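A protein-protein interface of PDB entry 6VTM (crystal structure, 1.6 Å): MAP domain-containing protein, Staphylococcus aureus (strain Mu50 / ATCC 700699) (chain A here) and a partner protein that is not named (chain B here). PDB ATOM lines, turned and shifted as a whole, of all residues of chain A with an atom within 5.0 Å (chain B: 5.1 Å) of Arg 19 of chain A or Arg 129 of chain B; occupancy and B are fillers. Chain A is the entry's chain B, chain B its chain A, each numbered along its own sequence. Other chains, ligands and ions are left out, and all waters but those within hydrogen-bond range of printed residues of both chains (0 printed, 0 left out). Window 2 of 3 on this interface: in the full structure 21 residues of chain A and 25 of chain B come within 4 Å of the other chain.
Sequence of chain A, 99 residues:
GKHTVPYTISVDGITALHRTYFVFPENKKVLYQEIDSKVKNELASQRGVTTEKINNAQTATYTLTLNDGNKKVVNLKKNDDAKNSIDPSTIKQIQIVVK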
ATOM      1  N   PRO A   6      19.633  18.810 -24.567  1.00  0.00           N
ATOM      2  CA  PRO A   6      20.272  18.524 -23.280  1.00  0.00           C
ATOM      3  C   PRO A   6      20.265  19.755 -22.405  1.00  0.00           C
ATOM      4  O   PRO A   6      20.366  20.878 -22.897  1.00  0.00           O
ATOM      5  CB  PRO A   6      21.707  18.137 -23.649  1.00  0.00           C
ATOM      6  CG  PRO A   6      21.705  17.879 -25.107  1.00  0.00           C
ATOM      7  CD  PRO A   6      20.525  18.588 -25.717  1.00  0.00           C
ATOM      8  N   THR A   8      21.614  21.137 -18.189  1.00  0.00           N
ATOM      9  CA  THR A   8      22.344  20.854 -16.959  1.00  0.00           C
ATOM     10  C   THR A   8      21.838  21.784 -15.873  1.00  0.00           C
ATOM     11  O   THR A   8      21.548  22.952 -16.129  1.00  0.00           O
ATOM     12  CB  THR A   8      23.863  21.048 -17.126  1.00  0.00           C
ATOM     13  OG1 THR A   8      24.360  20.155 -18.139  1.00  0.00           O
ATOM     14  CG2 THR A   8      24.586  20.773 -15.807  1.00  0.00           C
ATOM     15  N   LEU A  17      24.946  14.143 -11.555  1.00  0.00           N
ATOM     16  CA  LEU A  17      25.653  13.659 -12.738  1.00  0.00           C
ATOM     17  C   LEU A  17      24.829  12.700 -13.601  1.00  0.00           C
ATOM     18  O   LEU A  17      25.409  11.898 -14.358  1.00  0.00           O
ATOM     19  CB  LEU A  17      27.007  13.054 -12.328  1.00  0.00           C
ATOM     20  CG  LEU A  17      28.022  14.091 -11.807  1.00  0.00           C
ATOM     21  CD1 LEU A  17      29.244  13.404 -11.267  1.00  0.00           C
ATOM     22  CD2 LEU A  17      28.399  15.086 -12.921  1.00  0.00           C
ATOM     23  N   HIS A  18      23.495  12.810 -13.570  1.00  0.00           N
ATOM     24  CA  HIS A  18      22.682  12.231 -14.635  1.00  0.00           C
ATOM     25  C   HIS A  18      22.817  13.071 -15.896  1.00  0.00           C
ATOM     26  O   HIS A  18      23.404  14.156 -15.889  1.00  0.00           O
ATOM     27  CB  HIS A  18      21.222  12.101 -14.241  1.00  0.00           C
ATOM     28  CG  HIS A  18      20.550  13.338 -13.725  1.00  0.00           C
ATOM     29  ND1 HIS A  18      21.168  14.556 -13.560  1.00  0.00           N
ATOM     30  CD2 HIS A  18      19.269  13.508 -13.314  1.00  0.00           C
ATOM     31  CE1 HIS A  18      20.291  15.424 -13.066  1.00  0.00           C
ATOM     32  NE2 HIS A  18      19.147  14.803 -12.887  1.00  0.00           N
ATOM     33  N   ARG A  19      22.304  12.544 -17.010  1.00  0.00           N
ATOM     34  CA  ARG A  19      22.238  13.307 -18.249  1.00  0.00           C
ATOM     35  C   ARG A  19      20.758  13.537 -18.506  1.00  0.00           C
ATOM     36  O   ARG A  19      19.989  12.574 -18.613  1.00  0.00           O
ATOM     37  CB  ARG A  19      22.899  12.539 -19.390  1.00  0.00           C
ATOM     38  CG  ARG A  19      22.796  13.169 -20.764  1.00  0.00           C
ATOM     39  CD  ARG A  19      23.463  14.500 -20.792  1.00  0.00           C
ATOM     40  NE  ARG A  19      23.779  14.930 -22.156  1.00  0.00           N
ATOM     41  CZ  ARG A  19      24.360  16.086 -22.452  1.00  0.00           C
ATOM     42  NH1 ARG A  19      24.663  16.944 -21.485  1.00  0.00           N
ATOM     43  NH2 ARG A  19      24.619  16.392 -23.712  1.00  0.00           N
ATOM     44  N   THR A  20      20.340  14.803 -18.538  1.00  0.00           N
ATOM     45  CA  THR A  20      18.940  15.177 -18.715  1.00  0.00           C
ATOM     46  C   THR A  20      18.711  15.920 -20.032  1.00  0.00           C
ATOM     47  O   THR A  20      19.543  16.717 -20.446  1.00  0.00           O
ATOM     48  CB  THR A  20      18.463  16.066 -17.549  1.00  0.00           C
ATOM     49  OG1 THR A  20      19.397  17.095 -17.288  1.00  0.00           O
ATOM     50  CG2 THR A  20      18.329  15.213 -16.280  1.00  0.00           C
ATOM     51  N   TYR A  21      17.584  15.636 -20.682  1.00  0.00           N
ATOM     52  CA  TYR A  21      17.184  16.319 -21.909  1.00  0.00           C
ATOM     53  C   TYR A  21      15.740  16.804 -21.827  1.00  0.00           C
ATOM     54  O   TYR A  21      14.863  16.120 -21.290  1.00  0.00           O
ATOM     55  CB  TYR A  21      17.276  15.378 -23.161  1.00  0.00           C
ATOM     56  CG  TYR A  21      18.466  14.486 -23.284  1.00  0.00           C
ATOM     57  CD1 TYR A  21      18.533  13.299 -22.582  1.00  0.00           C
ATOM     58  CD2 TYR A  21      19.503  14.798 -24.150  1.00  0.00           C
ATOM     59  CE1 TYR A  21      19.629  12.473 -22.687  1.00  0.00           C
ATOM     60  CE2 TYR A  21      20.612  13.983 -24.260  1.00  0.00           C
ATOM     61  CZ  TYR A  21      20.661  12.815 -23.534  1.00  0.00           C
ATOM     62  OH  TYR A  21      21.740  11.974 -23.640  1.00  0.00           O
ATOM     63  N   GLN A  93      21.524  23.472 -26.433  1.00  0.00           N
ATOM     64  CA  GLN A  93      21.544  23.021 -25.046  1.00  0.00           C
ATOM     65  C   GLN A  93      21.276  24.192 -24.114  1.00  0.00           C
ATOM     66  O   GLN A  93      21.346  25.361 -24.506  1.00  0.00           O
ATOM     67  CB  GLN A  93      22.859  22.338 -24.695  1.00  0.00           C
ATOM     68  CG  GLN A  93      24.062  23.198 -24.755  1.00  0.00           C
ATOM     69  CD  GLN A  93      25.310  22.415 -24.388  1.00  0.00           C
ATOM     70  OE1 GLN A  93      25.342  21.164 -24.441  1.00  0.00           O
ATOM     71  NE2 GLN A  93      26.309  23.137 -23.880  1.00  0.00           N
ATOM     72  N   ILE B   1      32.224   9.310 -18.900  1.00  0.00           N
ATOM     73  CA  ILE B   1      33.530   9.179 -18.235  1.00  0.00           C
ATOM     74  C   ILE B   1      34.539  10.097 -18.894  1.00  0.00           C
ATOM     75  O   ILE B   1      34.725  10.005 -20.087  1.00  0.00           O
ATOM     76  CB  ILE B   1      34.031   7.726 -18.301  1.00  0.00           C
ATOM     77  CG1 ILE B   1      33.089   6.801 -17.539  1.00  0.00           C
ATOM     78  CG2 ILE B   1      35.460   7.594 -17.762  1.00  0.00           C
ATOM     79  CD1 ILE B   1      33.100   6.996 -16.045  1.00  0.00           C
ATOM     80  N   ILE B   2      35.172  10.977 -18.120  1.00  0.00           N
ATOM     81  CA  ILE B   2      36.223  11.861 -18.611  1.00  0.00           C
ATOM     82  C   ILE B   2      37.578  11.195 -18.396  1.00  0.00           C
ATOM     83  O   ILE B   2      37.877  10.712 -17.306  1.00  0.00           O
ATOM     84  CB  ILE B   2      36.167  13.217 -17.890  1.00  0.00           C
ATOM     85  CG1 ILE B   2      34.968  14.039 -18.379  1.00  0.00           C
ATOM     86  CG2 ILE B   2      37.452  13.987 -18.132  1.00  0.00           C
ATOM     87  CD1 ILE B   2      34.647  15.262 -17.539  1.00  0.00           C
ATOM     88  N   GLN B  26      13.572  13.322 -20.869  1.00  0.00           N
ATOM     89  CA  GLN B  26      14.051  12.041 -20.383  1.00  0.00           C
ATOM     90  C   GLN B  26      15.408  12.219 -19.740  1.00  0.00           C
ATOM     91  O   GLN B  26      16.066  13.245 -19.915  1.00  0.00           O
ATOM     92  CB  GLN B  26      14.150  11.017 -21.498  1.00  0.00           C
ATOM     93  CG  GLN B  26      12.797  10.561 -21.946  1.00  0.00           C
ATOM     94  CD  GLN B  26      12.864   9.352 -22.831  1.00  0.00           C
ATOM     95  OE1 GLN B  26      13.944   8.940 -23.243  1.00  0.00           O
ATOM     96  NE2 GLN B  26      11.710   8.737 -23.091  1.00  0.00           N
ATOM     97  N   SER B  27      15.831  11.201 -18.996  1.00  0.00           N
ATOM     98  CA  SER B  27      17.170  11.214 -18.440  1.00  0.00           C
ATOM     99  C   SER B  27      17.837   9.874 -18.695  1.00  0.00           C
ATOM    100  O   SER B  27      17.194   8.889 -19.056  1.00  0.00           O
ATOM    101  CB  SER B  27      17.200  11.559 -16.941  1.00  0.00           C
ATOM    102  OG  SER B  27      16.374  10.749 -16.165  1.00  0.00           O
ATOM    103  N   ARG B  28      19.207   9.965 -18.514  1.00  0.00           N
ATOM    104  CA  ARG B  28      19.981   8.748 -18.686  1.00  0.00           C
ATOM    105  C   ARG B  28      20.904   8.576 -17.502  1.00  0.00           C
ATOM    106  O   ARG B  28      21.468   9.543 -16.979  1.00  0.00           O
ATOM    107  CB  ARG B  28      20.792   8.726 -19.947  1.00  0.00           C
ATOM    108  CG  ARG B  28      20.085   8.833 -21.207  1.00  0.00           C
ATOM    109  CD  ARG B  28      19.332   7.522 -21.480  1.00  0.00           C
ATOM    110  NE  ARG B  28      18.620   7.511 -22.758  1.00  0.00           N
ATOM    111  CZ  ARG B  28      17.347   7.882 -22.911  1.00  0.00           C
ATOM    112  NH1 ARG B  28      16.624   8.292 -21.867  1.00  0.00           N
ATOM    113  NH2 ARG B  28      16.788   7.831 -24.111  1.00  0.00           N
ATOM    114  N   TRP B 127      28.491   5.072 -19.369  1.00  0.00           N
ATOM    115  CA  TRP B 127      28.201   5.501 -20.728  1.00  0.00           C
ATOM    116  C   TRP B 127      27.982   7.009 -20.820  1.00  0.00           C
ATOM    117  O   TRP B 127      27.369   7.494 -21.775  1.00  0.00           O
ATOM    118  CB  TRP B 127      26.966   4.754 -21.244  1.00  0.00           C
ATOM    119  CG  TRP B 127      27.131   3.278 -21.538  1.00  0.00           C
ATOM    120  CD1 TRP B 127      27.571   2.721 -22.707  1.00  0.00           C
ATOM    121  CD2 TRP B 127      26.824   2.185 -20.671  1.00  0.00           C
ATOM    122  NE1 TRP B 127      27.575   1.351 -22.613  1.00  0.00           N
ATOM    123  CE2 TRP B 127      27.112   0.995 -21.375  1.00  0.00           C
ATOM    124  CE3 TRP B 127      26.341   2.097 -19.368  1.00  0.00           C
ATOM    125  CZ2 TRP B 127      26.926  -0.270 -20.810  1.00  0.00           C
ATOM    126  CZ3 TRP B 127      26.149   0.859 -18.822  1.00  0.00           C
ATOM    127  CH2 TRP B 127      26.444  -0.319 -19.544  1.00  0.00           C
ATOM    128  N   GLY B 128      28.446   7.762 -19.843  1.00  0.00           N
ATOM    129  CA  GLY B 128      28.218   9.184 -19.813  1.00  0.00           C
ATOM    130  C   GLY B 128      29.089   9.900 -20.826  1.00  0.00           C
ATOM    131  O   GLY B 128      29.933   9.312 -21.500  1.00  0.00           O
ATOM    132  N   ARG B 129      28.895  11.214 -20.894  1.00  0.00           N
ATOM    133  CA  ARG B 129      29.695  12.053 -21.769  1.00  0.00           C
ATOM    134  C   ARG B 129      31.173  12.015 -21.393  1.00  0.00           C
ATOM    135  O   ARG B 129      31.554  11.833 -20.231  1.00  0.00           O
ATOM    136  CB  ARG B 129      29.172  13.493 -21.728  1.00  0.00           C
ATOM    137  CG  ARG B 129      27.660  13.642 -21.872  1.00  0.00           C
ATOM    138  CD  ARG B 129      27.176  13.225 -23.212  1.00  0.00           C
ATOM    139  NE  ARG B 129      27.560  14.189 -24.229  1.00  0.00           N
ATOM    140  CZ  ARG B 129      27.234  14.082 -25.517  1.00  0.00           C
ATOM    141  NH1 ARG B 129      26.525  13.038 -25.942  1.00  0.00           N
ATOM    142  NH2 ARG B 129      27.618  15.013 -26.371  1.00  0.00           N
ATOM    143  N   VAL B 130      32.024  12.234 -22.400  1.00  0.00           N
ATOM    144  CA  VAL B 130      33.477  12.161 -22.227  1.00  0.00           C
ATOM    145  C   VAL B 130      34.147  13.528 -22.283  1.00  0.00           C
ATOM    146  O   VAL B 130      35.356  13.639 -21.987  1.00  0.00           O
ATOM    147  CB  VAL B 130      34.096  11.214 -23.268  1.00  0.00           C
ATOM    148  CG1 VAL B 130      33.373   9.882 -23.256  1.00  0.00           C
ATOM    149  CG2 VAL B 130      34.103  11.852 -24.648  1.00  0.00           C
ATOM    150  N   SER B 131      33.395  14.569 -22.611  1.00  0.00           N
ATOM    151  CA  SER B 131      33.869  15.941 -22.662  1.00  0.00           C
ATOM    152  C   SER B 131      32.638  16.840 -22.763  1.00  0.00           C
ATOM    153  O   SER B 131      31.494  16.372 -22.736  1.00  0.00           O
ATOM    154  CB  SER B 131      34.785  16.154 -23.860  1.00  0.00           C
ATOM    155  OG  SER B 131      34.020  16.216 -25.063  1.00  0.00           O
ATOM    156  N   ARG B 133      31.723  18.206 -25.378  1.00  0.00           N
ATOM    157  CA  ARG B 133      31.260  18.147 -26.753  1.00  0.00           C
ATOM    158  C   ARG B 133      30.899  16.757 -27.237  1.00  0.00           C
ATOM    159  O   ARG B 133      30.217  16.640 -28.261  1.00  0.00           O
ATOM    160  CB  ARG B 133      32.336  18.713 -27.707  1.00  0.00           C
ATOM    161  CG  ARG B 133      31.929  18.759 -29.192  1.00  0.00           C
ATOM    162  CD  ARG B 133      33.040  19.405 -30.071  1.00  0.00           C
ATOM    163  NE  ARG B 133      34.288  18.646 -30.024  1.00  0.00           N
ATOM    164  CZ  ARG B 133      34.536  17.596 -30.796  1.00  0.00           C
ATOM    165  NH1 ARG B 133      33.594  17.185 -31.652  1.00  0.00           N
ATOM    166  NH2 ARG B 133      35.685  16.926 -30.694  1.00  0.00           N
ATOM    167  N   ARG B 134      31.347  15.695 -26.566  1.00  0.00           N
ATOM    168  CA  ARG B 134      31.145  14.382 -27.138  1.00  0.00           C
ATOM    169  C   ARG B 134      30.759  13.385 -26.067  1.00  0.00           C
ATOM    170  O   ARG B 134      31.071  13.558 -24.886  1.00  0.00           O
ATOM    171  CB  ARG B 134      32.357  13.814 -27.876  1.00  0.00           C
ATOM    172  CG  ARG B 134      33.696  14.018 -27.302  1.00  0.00           C
ATOM    173  CD  ARG B 134      34.745  13.985 -28.443  1.00  0.00           C
ATOM    174  NE  ARG B 134      36.049  13.763 -27.860  1.00  0.00           N
ATOM    175  CZ  ARG B 134      36.543  12.559 -27.605  1.00  0.00           C
ATOM    176  NH1 ARG B 134      35.845  11.474 -27.909  1.00  0.00           N
ATOM    177  NH2 ARG B 134      37.740  12.436 -27.053  1.00  0.00           N
ATOM    178  N   GLY B 135      30.075  12.340 -26.526  1.00  0.00           N
ATOM    179  CA  GLY B 135      29.691  11.225 -25.724  1.00  0.00           C
ATOM    180  C   GLY B 135      30.337   9.955 -26.225  1.00  0.00           C
ATOM    181  O   GLY B 135      31.328   9.977 -26.966  1.00  0.00           O
ATOM    182  N   PHE B 177      31.182  11.641 -15.206  1.00  0.00           N
ATOM    183  CA  PHE B 177      30.553  12.844 -15.761  1.00  0.00           C
ATOM    184  C   PHE B 177      29.090  12.566 -16.097  1.00  0.00           C
ATOM    185  O   PHE B 177      28.486  11.612 -15.602  1.00  0.00           O
ATOM    186  CB  PHE B 177      31.374  13.337 -16.957  1.00  0.00           C
ATOM    187  CG  PHE B 177      31.158  14.787 -17.312  1.00  0.00           C
ATOM    188  CD1 PHE B 177      31.076  15.768 -16.331  1.00  0.00           C
ATOM    189  CD2 PHE B 177      31.039  15.148 -18.614  1.00  0.00           C
ATOM    190  CE1 PHE B 177      30.881  17.089 -16.660  1.00  0.00           C
ATOM    191  CE2 PHE B 177      30.850  16.476 -18.951  1.00  0.00           C
ATOM    192  CZ  PHE B 177      30.779  17.444 -17.946  1.00  0.00           C
ATOM    193  N   LYS B 178      28.485  13.465 -16.880  1.00  0.00           N
ATOM    194  CA  LYS B 178      27.034  13.488 -17.068  1.00  0.00           C
ATOM    195  C   LYS B 178      26.551  12.239 -17.773  1.00  0.00           C
ATOM    196  O   LYS B 178      26.917  11.961 -18.918  1.00  0.00           O
ATOM    197  CB  LYS B 178      26.620  14.727 -17.846  1.00  0.00           C
ATOM    198  CG  LYS B 178      27.110  15.971 -17.176  1.00  0.00           C
ATOM    199  CD  LYS B 178      26.796  17.219 -17.980  1.00  0.00           C
ATOM    200  CE  LYS B 178      27.048  18.468 -17.129  1.00  0.00           C
ATOM    201  NZ  LYS B 178      27.541  19.629 -17.926  1.00  0.00           N
ATOM    202  N   GLY B 179      25.669  11.513 -17.099  1.00  0.00           N
ATOM    203  CA  GLY B 179      25.202  10.232 -17.549  1.00  0.00           C
ATOM    204  C   GLY B 179      25.842   9.057 -16.831  1.00  0.00           C
ATOM    205  O   GLY B 179      25.366   7.917 -16.983  1.00  0.00           O
ATOM    206  N   ASP B 180      26.878   9.311 -16.035  1.00  0.00           N
ATOM    207  CA  ASP B 180      27.490   8.249 -15.241  1.00  0.00           C
ATOM    208  C   ASP B 180      26.881   8.087 -13.849  1.00  0.00           C
ATOM    209  O   ASP B 180      27.222   7.108 -13.151  1.00  0.00           O
ATOM    210  CB  ASP B 180      28.988   8.506 -15.065  1.00  0.00           C
ATOM    211  CG  ASP B 180      29.744   8.442 -16.362  1.00  0.00           C
ATOM    212  OD1 ASP B 180      29.427   7.589 -17.252  1.00  0.00           O
ATOM    213  OD2 ASP B 180      30.652   9.291 -16.515  1.00  0.00           O
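The backbone carbonyl oxygen (O) of Gln 26 of chain B sits at hydrogen-bond distance from the backbone NH (N) of Tyr 21 of chain A (2.9 Å).
The backbone NH (N) of Arg 28 of chain B sits at hydrogen-bond distance from the backbone carbonyl oxygen (O) of Arg 19 of chain A, at 2.7 Å.
The side-chain hydroxyl (OG1) of Thr 8 of chain A sits at hydrogen-bond distance from the side-chain amino group (NZ) of Lys 178 of chain B, 3.2 Å away.
The backbone NH (N) of Gly 179 of chain B is in hydrogen-bond range of the backbone carbonyl oxygen (O) of Leu 17 of chain A (2.8 Å).
O of Leu 17 of chain A lies within hydrogen-bond range of N of Asp 180 of chain B, 3.4 Å away.
The backbone carbonyl oxygen (O) of Phe 177 of chain B lies close to the backbone carbonyl oxygen (O) of Leu 17 of chain A, 3.3 Å away.
The backbone NH of Ile 1 of chain B is in hydrogen-bond range of the backbone carbonyl oxygen of Arg 129 of chain B.
OE1 of Gln 26 of chain B lies within hydrogen-bond range of NH1 of Arg 28 of chain B, at 3.1 Å.
N of Trp 127 of chain B sits at hydrogen-bond distance from OD1 of Asp 180 of chain B (3.4 Å).
The backbone NH (N) of Gly 128 of chain B lies within hydrogen-bond range of the side-chain carboxylate (OD1) of Asp 180 of chain B (2.8 Å).
The backbone NH (N) of Arg 129 of chain B lies within hydrogen-bond range of the backbone carbonyl oxygen (O) of Lys 178 of chain B (2.9 Å).
The backbone NH (N) of Phe 177 of chain B is in hydrogen-bond range of the side-chain carboxylate (OD2) of Asp 180 of chain B (2.7 Å).
Among the printed residues, merely in contact across the chains: Leu 17 of chain A with Lys 178 of chain B, His 18 of chain A with Arg 28 of chain B, His 18 of chain A with Lys 178 of chain B, His 18 of chain A with Gly 179 of chain B, Arg 19 of chain A with Ser 27 of chain B, Arg 19 of chain A with Arg 129 of chain B, Arg 19 of chain A with Gly 179 of chain B, Thr 20 of chain A with Gln 26 of chain B, Thr 20 of chain A with Ser 27 of chain B and Tyr 21 of chain A with Arg 28 of chain B.
Arg 129 of chain B touches one residue of chain A.
Printed residues of chain B within 4 Å of Thr 20 of chain A: Gln 26 and Ser 27.
Of the printed residues of chain A, Asp 180 of chain B touches Leu 17.
Ile 1 of chain B touches none of the printed residues of chain A.
The nearest printed residue of chain B that does not touch Arg 19 of chain A is Lys 178 of chain B (4.01 Å).
The nearest printed residue of chain A that does not touch Arg 129 of chain B is Tyr 21 of chain A (5.4 Å).
Of the 8 printed residues of chain A, 6 touch a printed residue of chain B.
Printed residues of chain A that touch a printed residue of chain B: Thr 8, Leu 17, His 18, Arg 19, Thr 20 and Tyr 21.
Hydrophobic or aromatic side chains of chain A within 4 Å of the printed part of chain B: Leu 17, His 18 and Tyr 21.
Among the printed residues, 16 pairs touch across the chains.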
